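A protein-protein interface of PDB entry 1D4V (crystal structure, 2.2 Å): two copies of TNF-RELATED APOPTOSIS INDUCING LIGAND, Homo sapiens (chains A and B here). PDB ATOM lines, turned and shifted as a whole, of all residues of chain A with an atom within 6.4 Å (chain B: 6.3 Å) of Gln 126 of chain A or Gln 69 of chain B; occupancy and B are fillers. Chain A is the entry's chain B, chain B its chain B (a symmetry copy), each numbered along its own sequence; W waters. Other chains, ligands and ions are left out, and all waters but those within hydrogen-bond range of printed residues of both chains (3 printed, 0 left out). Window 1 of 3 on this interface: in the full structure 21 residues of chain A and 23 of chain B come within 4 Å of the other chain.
The side-chain amide nitrogen (NE2) of Gln 69 of chain B is in hydrogen-bond range of the side-chain amide oxygen (OE1) of Gln 126 of chain A, at 3.0 Å.
NE2 of Gln 69 of chain B lies within hydrogen-bond range of O of Lys 106 of chain A (3.0 Å).
OH of Tyr 125 of chain B sits at hydrogen-bond distance from OH of Tyr 65 of chain A, 2.6 Å away.
N of Lys 106 of chain A lies within hydrogen-bond range of O of Glu 153 of chain B (3.0 Å).
The backbone NH of Ala 108 of chain A lies within hydrogen-bond range of the side-chain hydroxyl of Ser 123 of chain B, at 2.8 Å.
N of Ser 68 of chain A sits at hydrogen-bond distance from O of Gln 126 of chain A, 3.1 Å away.
The backbone NH (N) of Tyr 71 of chain B lies within hydrogen-bond range of the side-chain hydroxyl (OG) of Ser 155 of chain B, at 3.1 Å.
N of Ile 66 of chain A lies within hydrogen-bond range of O of Gly 128 of chain A, 2.9 Å away.
OH of Tyr 125 of chain A sits at hydrogen-bond distance from OH of Tyr 65 of chain A (2.6 Å).
N of Gln 90 of chain A sits at hydrogen-bond distance from O of Ser 107 of chain A (2.9 Å).
N of Ile 92 of chain A is in hydrogen-bond range of O of Met 105 of chain A (2.9 Å).
Glu 153 of chain B touches Met 105 of chain A.
Met 105 of chain A touches Phe 156 of chain B (CG to CE2, 3.8 Å).
Gln 69 of chain B touches Ser 107 of chain A (OE1 to OG, 3.8 Å).
Ser 123 of chain B touches Ser 107 of chain A.
Tyr 71 of chain B touches Ala 108 of chain A.
Ser 123 of chain B touches Arg 109 of chain A.
Tyr 125 of chain B touches Tyr 125 of chain A.
CE1 of Tyr 67 of chain B touches O of Gly 127 of chain A, 3.9 Å away.
Gly 127 of chain A touches Tyr 125 of chain B.
Phe 156 of chain B touches Gly 127 of chain A.
Gln 126 of chain A touches one residue of chain B.
Of chain A, only Lys 106 (3.0 Å), Ser 107 (3.8 Å) and Gln 126 (3.0 Å) come within 4 Å of Gln 69 of chain B.
Of the printed residues of chain A, Ser 123 of chain B touches Ser 107 (3.1 Å), Ala 108 (2.8 Å) and Arg 109 (3.5 Å).
Printed residues of chain A within 4 Å of Tyr 71 of chain B: Ala 108.
Tyr 91 of chain A touches none of the printed residues of chain B.
Tyr 67 of chain A touches none of the printed residues of chain B.
The nearest residue of chain B that does not touch Gln 126 of chain A is Tyr 125 of chain B (4.4 Å).
Printed residues of chain B that touch a printed residue of chain A: Tyr 67, Gln 69, Tyr 71, Ser 123, Tyr 125, Glu 153 and Phe 156.
Hydrophobic or aromatic side chains of chain B that line the printed part of chain A: Tyr 67, Tyr 71, Tyr 125 and Phe 156.
Hydrophobic or aromatic side chains of chain A within 4 Å of the printed part of chain B: Tyr 65, Met 105, Ala 108 and Tyr 125.
Among the printed residues, no Asp or Glu carboxylate lies within 4 Å of a Lys or Arg side-chain nitrogen of the other chain.
Tyr 125 of chain B touches its own counterpart, Tyr 125 of chain A.
Gln 126 of chain A touches Gln 69 of chain B, but with the chains exchanged Gln 69 of chain A does not touch Gln 126 of chain B (10.9 Å).
Water W3 lies within hydrogen-bond range of the side-chain amide oxygen (OE1) of Gln 69 of chain B (2.6 Å), the side-chain hydroxyl (OG) of Ser 107 of chain A (2.6 Å), the backbone carbonyl oxygen (O) of Tyr 125 of chain A (2.7 Å) and the guanidinium group (NH2) of Arg 109 of chain A (3.3 Å).
Water W2 lies within hydrogen-bond range of OG of Ser 123 of chain B (2.6 Å), O of Ala 154 of chain B (2.8 Å), O of Lys 106 of chain A (2.8 Å) and NE2 of Gln 69 of chain B (3.3 Å).
Water W1 bridges N of Tyr 125 of chain B and NH2 of Arg 109 of chain A.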
ATOM      1  N   TYR A  65      25.121  35.169  -5.230  1.00  0.00           N
ATOM      2  CA  TYR A  65      25.372  33.849  -4.689  1.00  0.00           C
ATOM      3  C   TYR A  65      24.506  33.896  -3.414  1.00  0.00           C
ATOM      4  O   TYR A  65      24.701  34.747  -2.563  1.00  0.00           O
ATOM      5  CB  TYR A  65      26.825  33.671  -4.281  1.00  0.00           C
ATOM      6  CG  TYR A  65      27.042  32.340  -3.581  1.00  0.00           C
ATOM      7  CD1 TYR A  65      27.227  31.158  -4.308  1.00  0.00           C
ATOM      8  CD2 TYR A  65      27.005  32.259  -2.184  1.00  0.00           C
ATOM      9  CE1 TYR A  65      27.382  29.892  -3.641  1.00  0.00           C
ATOM     10  CE2 TYR A  65      27.137  31.018  -1.513  1.00  0.00           C
ATOM     11  CZ  TYR A  65      27.332  29.844  -2.247  1.00  0.00           C
ATOM     12  OH  TYR A  65      27.486  28.638  -1.577  1.00  0.00           O
ATOM     13  N   ILE A  66      23.550  33.003  -3.275  1.00  0.00           N
ATOM     14  CA  ILE A  66      22.673  33.012  -2.104  1.00  0.00           C
ATOM     15  C   ILE A  66      22.917  31.718  -1.343  1.00  0.00           C
ATOM     16  O   ILE A  66      23.071  30.674  -1.965  1.00  0.00           O
ATOM     17  CB  ILE A  66      21.174  33.014  -2.535  1.00  0.00           C
ATOM     18  CG1 ILE A  66      20.906  34.155  -3.492  1.00  0.00           C
ATOM     19  CG2 ILE A  66      20.269  33.120  -1.334  1.00  0.00           C
ATOM     20  CD1 ILE A  66      19.529  34.040  -4.147  1.00  0.00           C
ATOM     21  N   TYR A  67      22.940  31.769  -0.016  1.00  0.00           N
ATOM     22  CA  TYR A  67      23.170  30.552   0.746  1.00  0.00           C
ATOM     23  C   TYR A  67      22.445  30.574   2.078  1.00  0.00           C
ATOM     24  O   TYR A  67      22.028  31.622   2.556  1.00  0.00           O
ATOM     25  CB  TYR A  67      24.668  30.381   0.986  1.00  0.00           C
ATOM     26  CG  TYR A  67      25.232  31.458   1.892  1.00  0.00           C
ATOM     27  CD1 TYR A  67      25.206  31.315   3.275  1.00  0.00           C
ATOM     28  CD2 TYR A  67      25.717  32.656   1.362  1.00  0.00           C
ATOM     29  CE1 TYR A  67      25.655  32.372   4.134  1.00  0.00           C
ATOM     30  CE2 TYR A  67      26.157  33.703   2.190  1.00  0.00           C
ATOM     31  CZ  TYR A  67      26.118  33.553   3.568  1.00  0.00           C
ATOM     32  OH  TYR A  67      26.504  34.595   4.369  1.00  0.00           O
ATOM     33  N   SER A  68      22.293  29.404   2.677  1.00  0.00           N
ATOM     34  CA  SER A  68      21.654  29.299   3.968  1.00  0.00           C
ATOM     35  C   SER A  68      22.049  28.011   4.653  1.00  0.00           C
ATOM     36  O   SER A  68      22.243  26.987   3.999  1.00  0.00           O
ATOM     37  CB  SER A  68      20.121  29.340   3.843  1.00  0.00           C
ATOM     38  OG  SER A  68      19.540  29.087   5.116  1.00  0.00           O
ATOM     39  N   GLN A  69      22.217  28.077   5.969  1.00  0.00           N
ATOM     40  CA  GLN A  69      22.507  26.885   6.742  1.00  0.00           C
ATOM     41  C   GLN A  69      21.402  26.803   7.778  1.00  0.00           C
ATOM     42  O   GLN A  69      21.095  27.782   8.463  1.00  0.00           O
ATOM     43  CB  GLN A  69      23.857  26.967   7.438  1.00  0.00           C
ATOM     44  CG  GLN A  69      24.147  25.765   8.256  1.00  0.00           C
ATOM     45  CD  GLN A  69      25.614  25.455   8.377  1.00  0.00           C
ATOM     46  OE1 GLN A  69      26.169  24.753   7.533  1.00  0.00           O
ATOM     47  NE2 GLN A  69      26.251  25.945   9.435  1.00  0.00           N
ATOM     48  N   GLN A  90      15.427  22.086   3.335  1.00  0.00           N
ATOM     49  CA  GLN A  90      15.643  23.516   3.367  1.00  0.00           C
ATOM     50  C   GLN A  90      15.333  24.062   1.984  1.00  0.00           C
ATOM     51  O   GLN A  90      15.914  23.613   0.990  1.00  0.00           O
ATOM     52  CB  GLN A  90      17.085  23.862   3.704  1.00  0.00           C
ATOM     53  CG  GLN A  90      17.286  25.388   3.840  1.00  0.00           C
ATOM     54  CD  GLN A  90      18.741  25.816   3.585  1.00  0.00           C
ATOM     55  OE1 GLN A  90      19.026  26.439   2.590  1.00  0.00           O
ATOM     56  NE2 GLN A  90      19.652  25.446   4.484  1.00  0.00           N
ATOM     57  N   TYR A  91      14.394  25.002   1.900  1.00  0.00           N
ATOM     58  CA  TYR A  91      14.061  25.596   0.595  1.00  0.00           C
ATOM     59  C   TYR A  91      14.461  27.049   0.540  1.00  0.00           C
ATOM     60  O   TYR A  91      14.357  27.777   1.529  1.00  0.00           O
ATOM     61  CB  TYR A  91      12.562  25.578   0.304  1.00  0.00           C
ATOM     62  CG  TYR A  91      11.894  24.243   0.423  1.00  0.00           C
ATOM     63  CD1 TYR A  91      11.372  23.817   1.633  1.00  0.00           C
ATOM     64  CD2 TYR A  91      11.786  23.399  -0.687  1.00  0.00           C
ATOM     65  CE1 TYR A  91      10.757  22.574   1.744  1.00  0.00           C
ATOM     66  CE2 TYR A  91      11.171  22.182  -0.588  1.00  0.00           C
ATOM     67  CZ  TYR A  91      10.657  21.771   0.629  1.00  0.00           C
ATOM     68  OH  TYR A  91      10.012  20.563   0.702  1.00  0.00           O
ATOM     69  N   ILE A  92      14.919  27.474  -0.624  1.00  0.00           N
ATOM     70  CA  ILE A  92      15.262  28.858  -0.818  1.00  0.00           C
ATOM     71  C   ILE A  92      14.425  29.343  -1.995  1.00  0.00           C
ATOM     72  O   ILE A  92      14.492  28.796  -3.117  1.00  0.00           O
ATOM     73  CB  ILE A  92      16.750  29.036  -1.067  1.00  0.00           C
ATOM     74  CG1 ILE A  92      17.517  28.611   0.191  1.00  0.00           C
ATOM     75  CG2 ILE A  92      17.059  30.514  -1.371  1.00  0.00           C
ATOM     76  CD1 ILE A  92      19.037  28.891   0.152  1.00  0.00           C
ATOM     77  N   MET A 105      16.247  26.840  -4.839  1.00  0.00           N
ATOM     78  CA  MET A 105      17.052  25.709  -4.410  1.00  0.00           C
ATOM     79  C   MET A 105      16.425  24.891  -3.295  1.00  0.00           C
ATOM     80  O   MET A 105      15.733  25.446  -2.467  1.00  0.00           O
ATOM     81  CB  MET A 105      18.418  26.209  -3.882  1.00  0.00           C
ATOM     82  CG  MET A 105      19.328  26.932  -4.831  1.00  0.00           C
ATOM     83  SD  MET A 105      20.866  27.576  -4.022  1.00  0.00           S
ATOM     84  CE  MET A 105      20.351  29.205  -3.411  1.00  0.00           C
ATOM     85  N   LYS A 106      16.658  23.569  -3.280  1.00  0.00           N
ATOM     86  CA  LYS A 106      16.212  22.727  -2.154  1.00  0.00           C
ATOM     87  C   LYS A 106      17.320  21.766  -1.799  1.00  0.00           C
ATOM     88  O   LYS A 106      18.102  21.376  -2.643  1.00  0.00           O
ATOM     89  CB  LYS A 106      14.911  21.922  -2.408  1.00  0.00           C
ATOM     90  CG  LYS A 106      14.852  21.018  -3.603  1.00  0.00           C
ATOM     91  CD  LYS A 106      13.539  20.175  -3.563  1.00  0.00           C
ATOM     92  CE  LYS A 106      13.466  19.145  -4.686  1.00  0.00           C
ATOM     93  NZ  LYS A 106      12.246  18.303  -4.507  1.00  0.00           N
ATOM     94  N   SER A 107      17.366  21.374  -0.542  1.00  0.00           N
ATOM     95  CA  SER A 107      18.372  20.457  -0.084  1.00  0.00           C
ATOM     96  C   SER A 107      17.715  19.671   1.001  1.00  0.00           C
ATOM     97  O   SER A 107      17.109  20.251   1.907  1.00  0.00           O
ATOM     98  CB  SER A 107      19.583  21.222   0.447  1.00  0.00           C
ATOM     99  OG  SER A 107      20.552  20.287   0.848  1.00  0.00           O
ATOM    100  N   ALA A 108      17.823  18.347   0.902  1.00  0.00           N
ATOM    101  CA  ALA A 108      17.130  17.473   1.832  1.00  0.00           C
ATOM    102  C   ALA A 108      17.936  16.381   2.502  1.00  0.00           C
ATOM    103  O   ALA A 108      18.945  15.930   1.986  1.00  0.00           O
ATOM    104  CB  ALA A 108      15.918  16.820   1.101  1.00  0.00           C
ATOM    105  N   ARG A 109      17.456  15.962   3.666  1.00  0.00           N
ATOM    106  CA  ARG A 109      18.065  14.867   4.413  1.00  0.00           C
ATOM    107  C   ARG A 109      16.891  14.121   5.032  1.00  0.00           C
ATOM    108  O   ARG A 109      15.830  14.704   5.274  1.00  0.00           O
ATOM    109  CB  ARG A 109      18.948  15.374   5.555  1.00  0.00           C
ATOM    110  CG  ARG A 109      19.895  16.496   5.199  1.00  0.00           C
ATOM    111  CD  ARG A 109      21.095  16.107   4.335  1.00  0.00           C
ATOM    112  NE  ARG A 109      21.586  17.318   3.651  1.00  0.00           N
ATOM    113  CZ  ARG A 109      22.766  17.893   3.877  1.00  0.00           C
ATOM    114  NH1 ARG A 109      23.610  17.375   4.760  1.00  0.00           N
ATOM    115  NH2 ARG A 109      23.096  19.012   3.243  1.00  0.00           N
ATOM    116  N   ILE A 124      22.218  21.614   7.431  1.00  0.00           N
ATOM    117  CA  ILE A 124      22.061  21.661   5.996  1.00  0.00           C
ATOM    118  C   ILE A 124      22.483  23.007   5.460  1.00  0.00           C
ATOM    119  O   ILE A 124      21.963  24.049   5.866  1.00  0.00           O
ATOM    120  CB  ILE A 124      20.589  21.408   5.555  1.00  0.00           C
ATOM    121  CG1 ILE A 124      20.176  19.968   5.915  1.00  0.00           C
ATOM    122  CG2 ILE A 124      20.472  21.560   4.043  1.00  0.00           C
ATOM    123  CD1 ILE A 124      18.681  19.669   5.657  1.00  0.00           C
ATOM    124  N   TYR A 125      23.457  22.973   4.557  1.00  0.00           N
ATOM    125  CA  TYR A 125      23.925  24.174   3.898  1.00  0.00           C
ATOM    126  C   TYR A 125      23.759  24.015   2.383  1.00  0.00           C
ATOM    127  O   TYR A 125      24.001  22.945   1.820  1.00  0.00           O
ATOM    128  CB  TYR A 125      25.419  24.420   4.194  1.00  0.00           C
ATOM    129  CG  TYR A 125      25.986  25.566   3.363  1.00  0.00           C
ATOM    130  CD1 TYR A 125      26.148  26.841   3.909  1.00  0.00           C
ATOM    131  CD2 TYR A 125      26.313  25.383   2.015  1.00  0.00           C
ATOM    132  CE1 TYR A 125      26.635  27.907   3.130  1.00  0.00           C
ATOM    133  CE2 TYR A 125      26.776  26.435   1.235  1.00  0.00           C
ATOM    134  CZ  TYR A 125      26.940  27.695   1.808  1.00  0.00           C
ATOM    135  OH  TYR A 125      27.441  28.717   1.034  1.00  0.00           O
ATOM    136  N   GLN A 126      23.316  25.062   1.714  1.00  0.00           N
ATOM    137  CA  GLN A 126      23.288  25.018   0.277  1.00  0.00           C
ATOM    138  C   GLN A 126      23.494  26.443  -0.207  1.00  0.00           C
ATOM    139  O   GLN A 126      23.272  27.375   0.537  1.00  0.00           O
ATOM    140  CB  GLN A 126      21.961  24.445  -0.249  1.00  0.00           C
ATOM    141  CG  GLN A 126      20.773  25.364  -0.200  1.00  0.00           C
ATOM    142  CD  GLN A 126      19.544  24.678  -0.690  1.00  0.00           C
ATOM    143  OE1 GLN A 126      19.627  23.898  -1.635  1.00  0.00           O
ATOM    144  NE2 GLN A 126      18.379  24.956  -0.062  1.00  0.00           N
ATOM    145  N   GLY A 127      23.917  26.609  -1.452  1.00  0.00           N
ATOM    146  CA  GLY A 127      24.088  27.946  -1.980  1.00  0.00           C
ATOM    147  C   GLY A 127      24.221  27.854  -3.492  1.00  0.00           C
ATOM    148  O   GLY A 127      24.511  26.781  -3.997  1.00  0.00           O
ATOM    149  N   GLY A 128      24.054  28.968  -4.201  1.00  0.00           N
ATOM    150  CA  GLY A 128      24.131  28.954  -5.656  1.00  0.00           C
ATOM    151  C   GLY A 128      23.878  30.340  -6.221  1.00  0.00           C
ATOM    152  O   GLY A 128      23.400  31.220  -5.502  1.00  0.00           O
ATOM    153  N   TRP B  36      23.691  18.815 -18.027  1.00  0.00           N
ATOM    154  CA  TRP B  36      23.358  20.180 -17.598  1.00  0.00           C
ATOM    155  C   TRP B  36      22.803  20.965 -18.794  1.00  0.00           C
ATOM    156  O   TRP B  36      23.236  20.755 -19.926  1.00  0.00           O
ATOM    157  CB  TRP B  36      24.602  20.893 -17.064  1.00  0.00           C
ATOM    158  CG  TRP B  36      25.334  20.139 -15.987  1.00  0.00           C
ATOM    159  CD1 TRP B  36      26.594  19.617 -16.062  1.00  0.00           C
ATOM    160  CD2 TRP B  36      24.870  19.879 -14.656  1.00  0.00           C
ATOM    161  NE1 TRP B  36      26.950  19.058 -14.855  1.00  0.00           N
ATOM    162  CE2 TRP B  36      25.913  19.203 -13.976  1.00  0.00           C
ATOM    163  CE3 TRP B  36      23.677  20.156 -13.970  1.00  0.00           C
ATOM    164  CZ2 TRP B  36      25.803  18.804 -12.637  1.00  0.00           C
ATOM    165  CZ3 TRP B  36      23.566  19.753 -12.634  1.00  0.00           C
ATOM    166  CH2 TRP B  36      24.626  19.086 -11.983  1.00  0.00           C
ATOM    167  N   TYR B  67      31.333  25.263  -7.345  1.00  0.00           N
ATOM    168  CA  TYR B  67      30.471  24.509  -6.450  1.00  0.00           C
ATOM    169  C   TYR B  67      29.482  23.646  -7.210  1.00  0.00           C
ATOM    170  O   TYR B  67      29.242  23.851  -8.394  1.00  0.00           O
ATOM    171  CB  TYR B  67      29.709  25.476  -5.545  1.00  0.00           C
ATOM    172  CG  TYR B  67      28.725  26.333  -6.317  1.00  0.00           C
ATOM    173  CD1 TYR B  67      27.433  25.885  -6.574  1.00  0.00           C
ATOM    174  CD2 TYR B  67      29.119  27.558  -6.861  1.00  0.00           C
ATOM    175  CE1 TYR B  67      26.534  26.654  -7.382  1.00  0.00           C
ATOM    176  CE2 TYR B  67      28.250  28.322  -7.658  1.00  0.00           C
ATOM    177  CZ  TYR B  67      26.966  27.862  -7.916  1.00  0.00           C
ATOM    178  OH  TYR B  67      26.142  28.588  -8.732  1.00  0.00           O
ATOM    179  N   SER B  68      28.908  22.673  -6.522  1.00  0.00           N
ATOM    180  CA  SER B  68      27.920  21.808  -7.124  1.00  0.00           C
ATOM    181  C   SER B  68      27.069  21.153  -6.062  1.00  0.00           C
ATOM    182  O   SER B  68      27.554  20.838  -4.975  1.00  0.00           O
ATOM    183  CB  SER B  68      28.580  20.708  -7.974  1.00  0.00           C
ATOM    184  OG  SER B  68      27.580  19.801  -8.423  1.00  0.00           O
ATOM    185  N   GLN B  69      25.784  20.995  -6.359  1.00  0.00           N
ATOM    186  CA  GLN B  69      24.893  20.298  -5.452  1.00  0.00           C
ATOM    187  C   GLN B  69      24.308  19.159  -6.267  1.00  0.00           C
ATOM    188  O   GLN B  69      23.831  19.354  -7.388  1.00  0.00           O
ATOM    189  CB  GLN B  69      23.773  21.194  -4.947  1.00  0.00           C
ATOM    190  CG  GLN B  69      22.837  20.480  -4.045  1.00  0.00           C
ATOM    191  CD  GLN B  69      22.191  21.368  -3.018  1.00  0.00           C
ATOM    192  OE1 GLN B  69      22.744  21.569  -1.937  1.00  0.00           O
ATOM    193  NE2 GLN B  69      21.006  21.886  -3.324  1.00  0.00           N
ATOM    194  N   THR B  70      24.355  17.962  -5.701  1.00  0.00           N
ATOM    195  CA  THR B  70      23.830  16.780  -6.376  1.00  0.00           C
ATOM    196  C   THR B  70      22.944  16.046  -5.396  1.00  0.00           C
ATOM    197  O   THR B  70      23.386  15.629  -4.344  1.00  0.00           O
ATOM    198  CB  THR B  70      24.966  15.828  -6.833  1.00  0.00           C
ATOM    199  OG1 THR B  70      24.385  14.608  -7.302  1.00  0.00           O
ATOM    200  CG2 THR B  70      25.884  15.500  -5.699  1.00  0.00           C
ATOM    201  N   TYR B  71      21.682  15.886  -5.773  1.00  0.00           N
ATOM    202  CA  TYR B  71      20.691  15.252  -4.931  1.00  0.00           C
ATOM    203  C   TYR B  71      20.482  13.752  -5.186  1.00  0.00           C
ATOM    204  O   TYR B  71      19.983  13.332  -6.236  1.00  0.00           O
ATOM    205  CB  TYR B  71      19.402  16.026  -5.117  1.00  0.00           C
ATOM    206  CG  TYR B  71      18.243  15.596  -4.285  1.00  0.00           C
ATOM    207  CD1 TYR B  71      18.427  15.014  -3.027  1.00  0.00           C
ATOM    208  CD2 TYR B  71      16.941  15.864  -4.717  1.00  0.00           C
ATOM    209  CE1 TYR B  71      17.333  14.717  -2.218  1.00  0.00           C
ATOM    210  CE2 TYR B  71      15.840  15.585  -3.921  1.00  0.00           C
ATOM    211  CZ  TYR B  71      16.039  15.023  -2.675  1.00  0.00           C
ATOM    212  OH  TYR B  71      14.954  14.880  -1.851  1.00  0.00           O
ATOM    213  N   GLN B  90      30.293  12.879  -4.703  1.00  0.00           N
ATOM    214  CA  GLN B  90      30.268  13.904  -5.724  1.00  0.00           C
ATOM    215  C   GLN B  90      31.700  14.344  -5.973  1.00  0.00           C
ATOM    216  O   GLN B  90      32.400  14.755  -5.041  1.00  0.00           O
ATOM    217  CB  GLN B  90      29.466  15.119  -5.285  1.00  0.00           C
ATOM    218  CG  GLN B  90      29.354  16.166  -6.417  1.00  0.00           C
ATOM    219  CD  GLN B  90      29.106  17.586  -5.883  1.00  0.00           C
ATOM    220  OE1 GLN B  90      29.970  18.426  -5.964  1.00  0.00           O
ATOM    221  NE2 GLN B  90      27.924  17.827  -5.317  1.00  0.00           N
ATOM    222  N   SER B 123      21.242  15.296  -0.197  1.00  0.00           N
ATOM    223  CA  SER B 123      21.719  16.397  -1.038  1.00  0.00           C
ATOM    224  C   SER B 123      23.167  16.651  -0.627  1.00  0.00           C
ATOM    225  O   SER B 123      23.476  16.774   0.567  1.00  0.00           O
ATOM    226  CB  SER B 123      20.920  17.705  -0.827  1.00  0.00           C
ATOM    227  OG  SER B 123      19.558  17.575  -1.222  1.00  0.00           O
ATOM    228  N   ILE B 124      24.051  16.704  -1.617  1.00  0.00           N
ATOM    229  CA  ILE B 124      25.449  16.969  -1.372  1.00  0.00           C
ATOM    230  C   ILE B 124      25.879  18.238  -2.066  1.00  0.00           C
ATOM    231  O   ILE B 124      25.742  18.379  -3.284  1.00  0.00           O
ATOM    232  CB  ILE B 124      26.365  15.813  -1.875  1.00  0.00           C
ATOM    233  CG1 ILE B 124      26.091  14.537  -1.056  1.00  0.00           C
ATOM    234  CG2 ILE B 124      27.828  16.190  -1.673  1.00  0.00           C
ATOM    235  CD1 ILE B 124      26.842  13.291  -1.582  1.00  0.00           C
ATOM    236  N   TYR B 125      26.378  19.175  -1.267  1.00  0.00           N
ATOM    237  CA  TYR B 125      26.898  20.420  -1.790  1.00  0.00           C
ATOM    238  C   TYR B 125      28.363  20.573  -1.368  1.00  0.00           C
ATOM    239  O   TYR B 125      28.743  20.244  -0.242  1.00  0.00           O
ATOM    240  CB  TYR B 125      26.109  21.624  -1.233  1.00  0.00           C
ATOM    241  CG  TYR B 125      26.751  22.955  -1.613  1.00  0.00           C
ATOM    242  CD1 TYR B 125      26.257  23.717  -2.672  1.00  0.00           C
ATOM    243  CD2 TYR B 125      27.886  23.422  -0.940  1.00  0.00           C
ATOM    244  CE1 TYR B 125      26.875  24.925  -3.046  1.00  0.00           C
ATOM    245  CE2 TYR B 125      28.511  24.605  -1.316  1.00  0.00           C
ATOM    246  CZ  TYR B 125      27.989  25.353  -2.370  1.00  0.00           C
ATOM    247  OH  TYR B 125      28.596  26.544  -2.702  1.00  0.00           O
ATOM    248  N   GLN B 126      29.202  21.041  -2.271  1.00  0.00           N
ATOM    249  CA  GLN B 126      30.553  21.348  -1.882  1.00  0.00           C
ATOM    250  C   GLN B 126      31.014  22.489  -2.772  1.00  0.00           C
ATOM    251  O   GLN B 126      30.449  22.705  -3.824  1.00  0.00           O
ATOM    252  CB  GLN B 126      31.479  20.128  -2.029  1.00  0.00           C
ATOM    253  CG  GLN B 126      31.902  19.779  -3.428  1.00  0.00           C
ATOM    254  CD  GLN B 126      32.754  18.555  -3.440  1.00  0.00           C
ATOM    255  OE1 GLN B 126      33.563  18.377  -2.534  1.00  0.00           O
ATOM    256  NE2 GLN B 126      32.592  17.690  -4.468  1.00  0.00           N
ATOM    257  N   GLU B 153      16.160  22.807  -9.204  1.00  0.00           N
ATOM    258  CA  GLU B 153      16.384  23.427  -7.903  1.00  0.00           C
ATOM    259  C   GLU B 153      17.214  22.474  -7.001  1.00  0.00           C
ATOM    260  O   GLU B 153      17.776  22.889  -5.988  1.00  0.00           O
ATOM    261  CB  GLU B 153      15.032  23.733  -7.217  1.00  0.00           C
ATOM    262  CG  GLU B 153      14.008  24.559  -8.091  1.00  0.00           C
ATOM    263  CD  GLU B 153      12.984  23.695  -8.871  1.00  0.00           C
ATOM    264  OE1 GLU B 153      13.341  22.611  -9.415  1.00  0.00           O
ATOM    265  OE2 GLU B 153      11.810  24.119  -8.956  1.00  0.00           O
ATOM    266  N   ALA B 154      17.273  21.210  -7.398  1.00  0.00           N
ATOM    267  CA  ALA B 154      17.944  20.146  -6.649  1.00  0.00           C
ATOM    268  C   ALA B 154      19.402  19.861  -6.955  1.00  0.00           C
ATOM    269  O   ALA B 154      20.183  19.606  -6.036  1.00  0.00           O
ATOM    270  CB  ALA B 154      17.157  18.828  -6.814  1.00  0.00           C
ATOM    271  N   SER B 155      19.737  19.834  -8.244  1.00  0.00           N
ATOM    272  CA  SER B 155      21.078  19.538  -8.677  1.00  0.00           C
ATOM    273  C   SER B 155      21.505  20.624  -9.601  1.00  0.00           C
ATOM    274  O   SER B 155      20.761  21.042 -10.475  1.00  0.00           O
ATOM    275  CB  SER B 155      21.139  18.173  -9.374  1.00  0.00           C
ATOM    276  OG  SER B 155      20.782  17.150  -8.443  1.00  0.00           O
ATOM    277  N   PHE B 156      22.708  21.118  -9.372  1.00  0.00           N
ATOM    278  CA  PHE B 156      23.207  22.189 -10.184  1.00  0.00           C
ATOM    279  C   PHE B 156      24.702  22.248 -10.060  1.00  0.00           C
ATOM    280  O   PHE B 156      25.284  21.542  -9.240  1.00  0.00           O
ATOM    281  CB  PHE B 156      22.547  23.512  -9.788  1.00  0.00           C
ATOM    282  CG  PHE B 156      22.517  23.773  -8.301  1.00  0.00           C
ATOM    283  CD1 PHE B 156      23.657  24.204  -7.622  1.00  0.00           C
ATOM    284  CD2 PHE B 156      21.322  23.666  -7.598  1.00  0.00           C
ATOM    285  CE1 PHE B 156      23.597  24.537  -6.260  1.00  0.00           C
ATOM    286  CE2 PHE B 156      21.245  23.992  -6.244  1.00  0.00           C
ATOM    287  CZ  PHE B 156      22.381  24.432  -5.563  1.00  0.00           C
ATOM    288  N   PHE B 157      25.303  23.120 -10.855  1.00  0.00           N
ATOM    289  CA  PHE B 157      26.739  23.257 -10.940  1.00  0.00           C
ATOM    290  C   PHE B 157      27.068  24.698 -11.331  1.00  0.00           C
ATOM    291  O   PHE B 157      26.466  25.237 -12.249  1.00  0.00           O
ATOM    292  CB  PHE B 157      27.164  22.268 -12.022  1.00  0.00           C
ATOM    293  CG  PHE B 157      28.612  22.305 -12.384  1.00  0.00           C
ATOM    294  CD1 PHE B 157      29.588  22.536 -11.429  1.00  0.00           C
ATOM    295  CD2 PHE B 157      28.997  22.002 -13.685  1.00  0.00           C
ATOM    296  CE1 PHE B 157      30.941  22.457 -11.756  1.00  0.00           C
ATOM    297  CE2 PHE B 157      30.340  21.916 -14.032  1.00  0.00           C
ATOM    298  CZ  PHE B 157      31.323  22.141 -13.063  1.00  0.00           C
HETATM  299  O   HOH W   1      26.089  18.859   1.685  1.00  0.00           O
HETATM  300  O   HOH W   2      19.446  19.015  -3.423  1.00  0.00           O
HETATM  301  O   HOH W   3      23.079  20.748   0.455  1.00  0.00           O
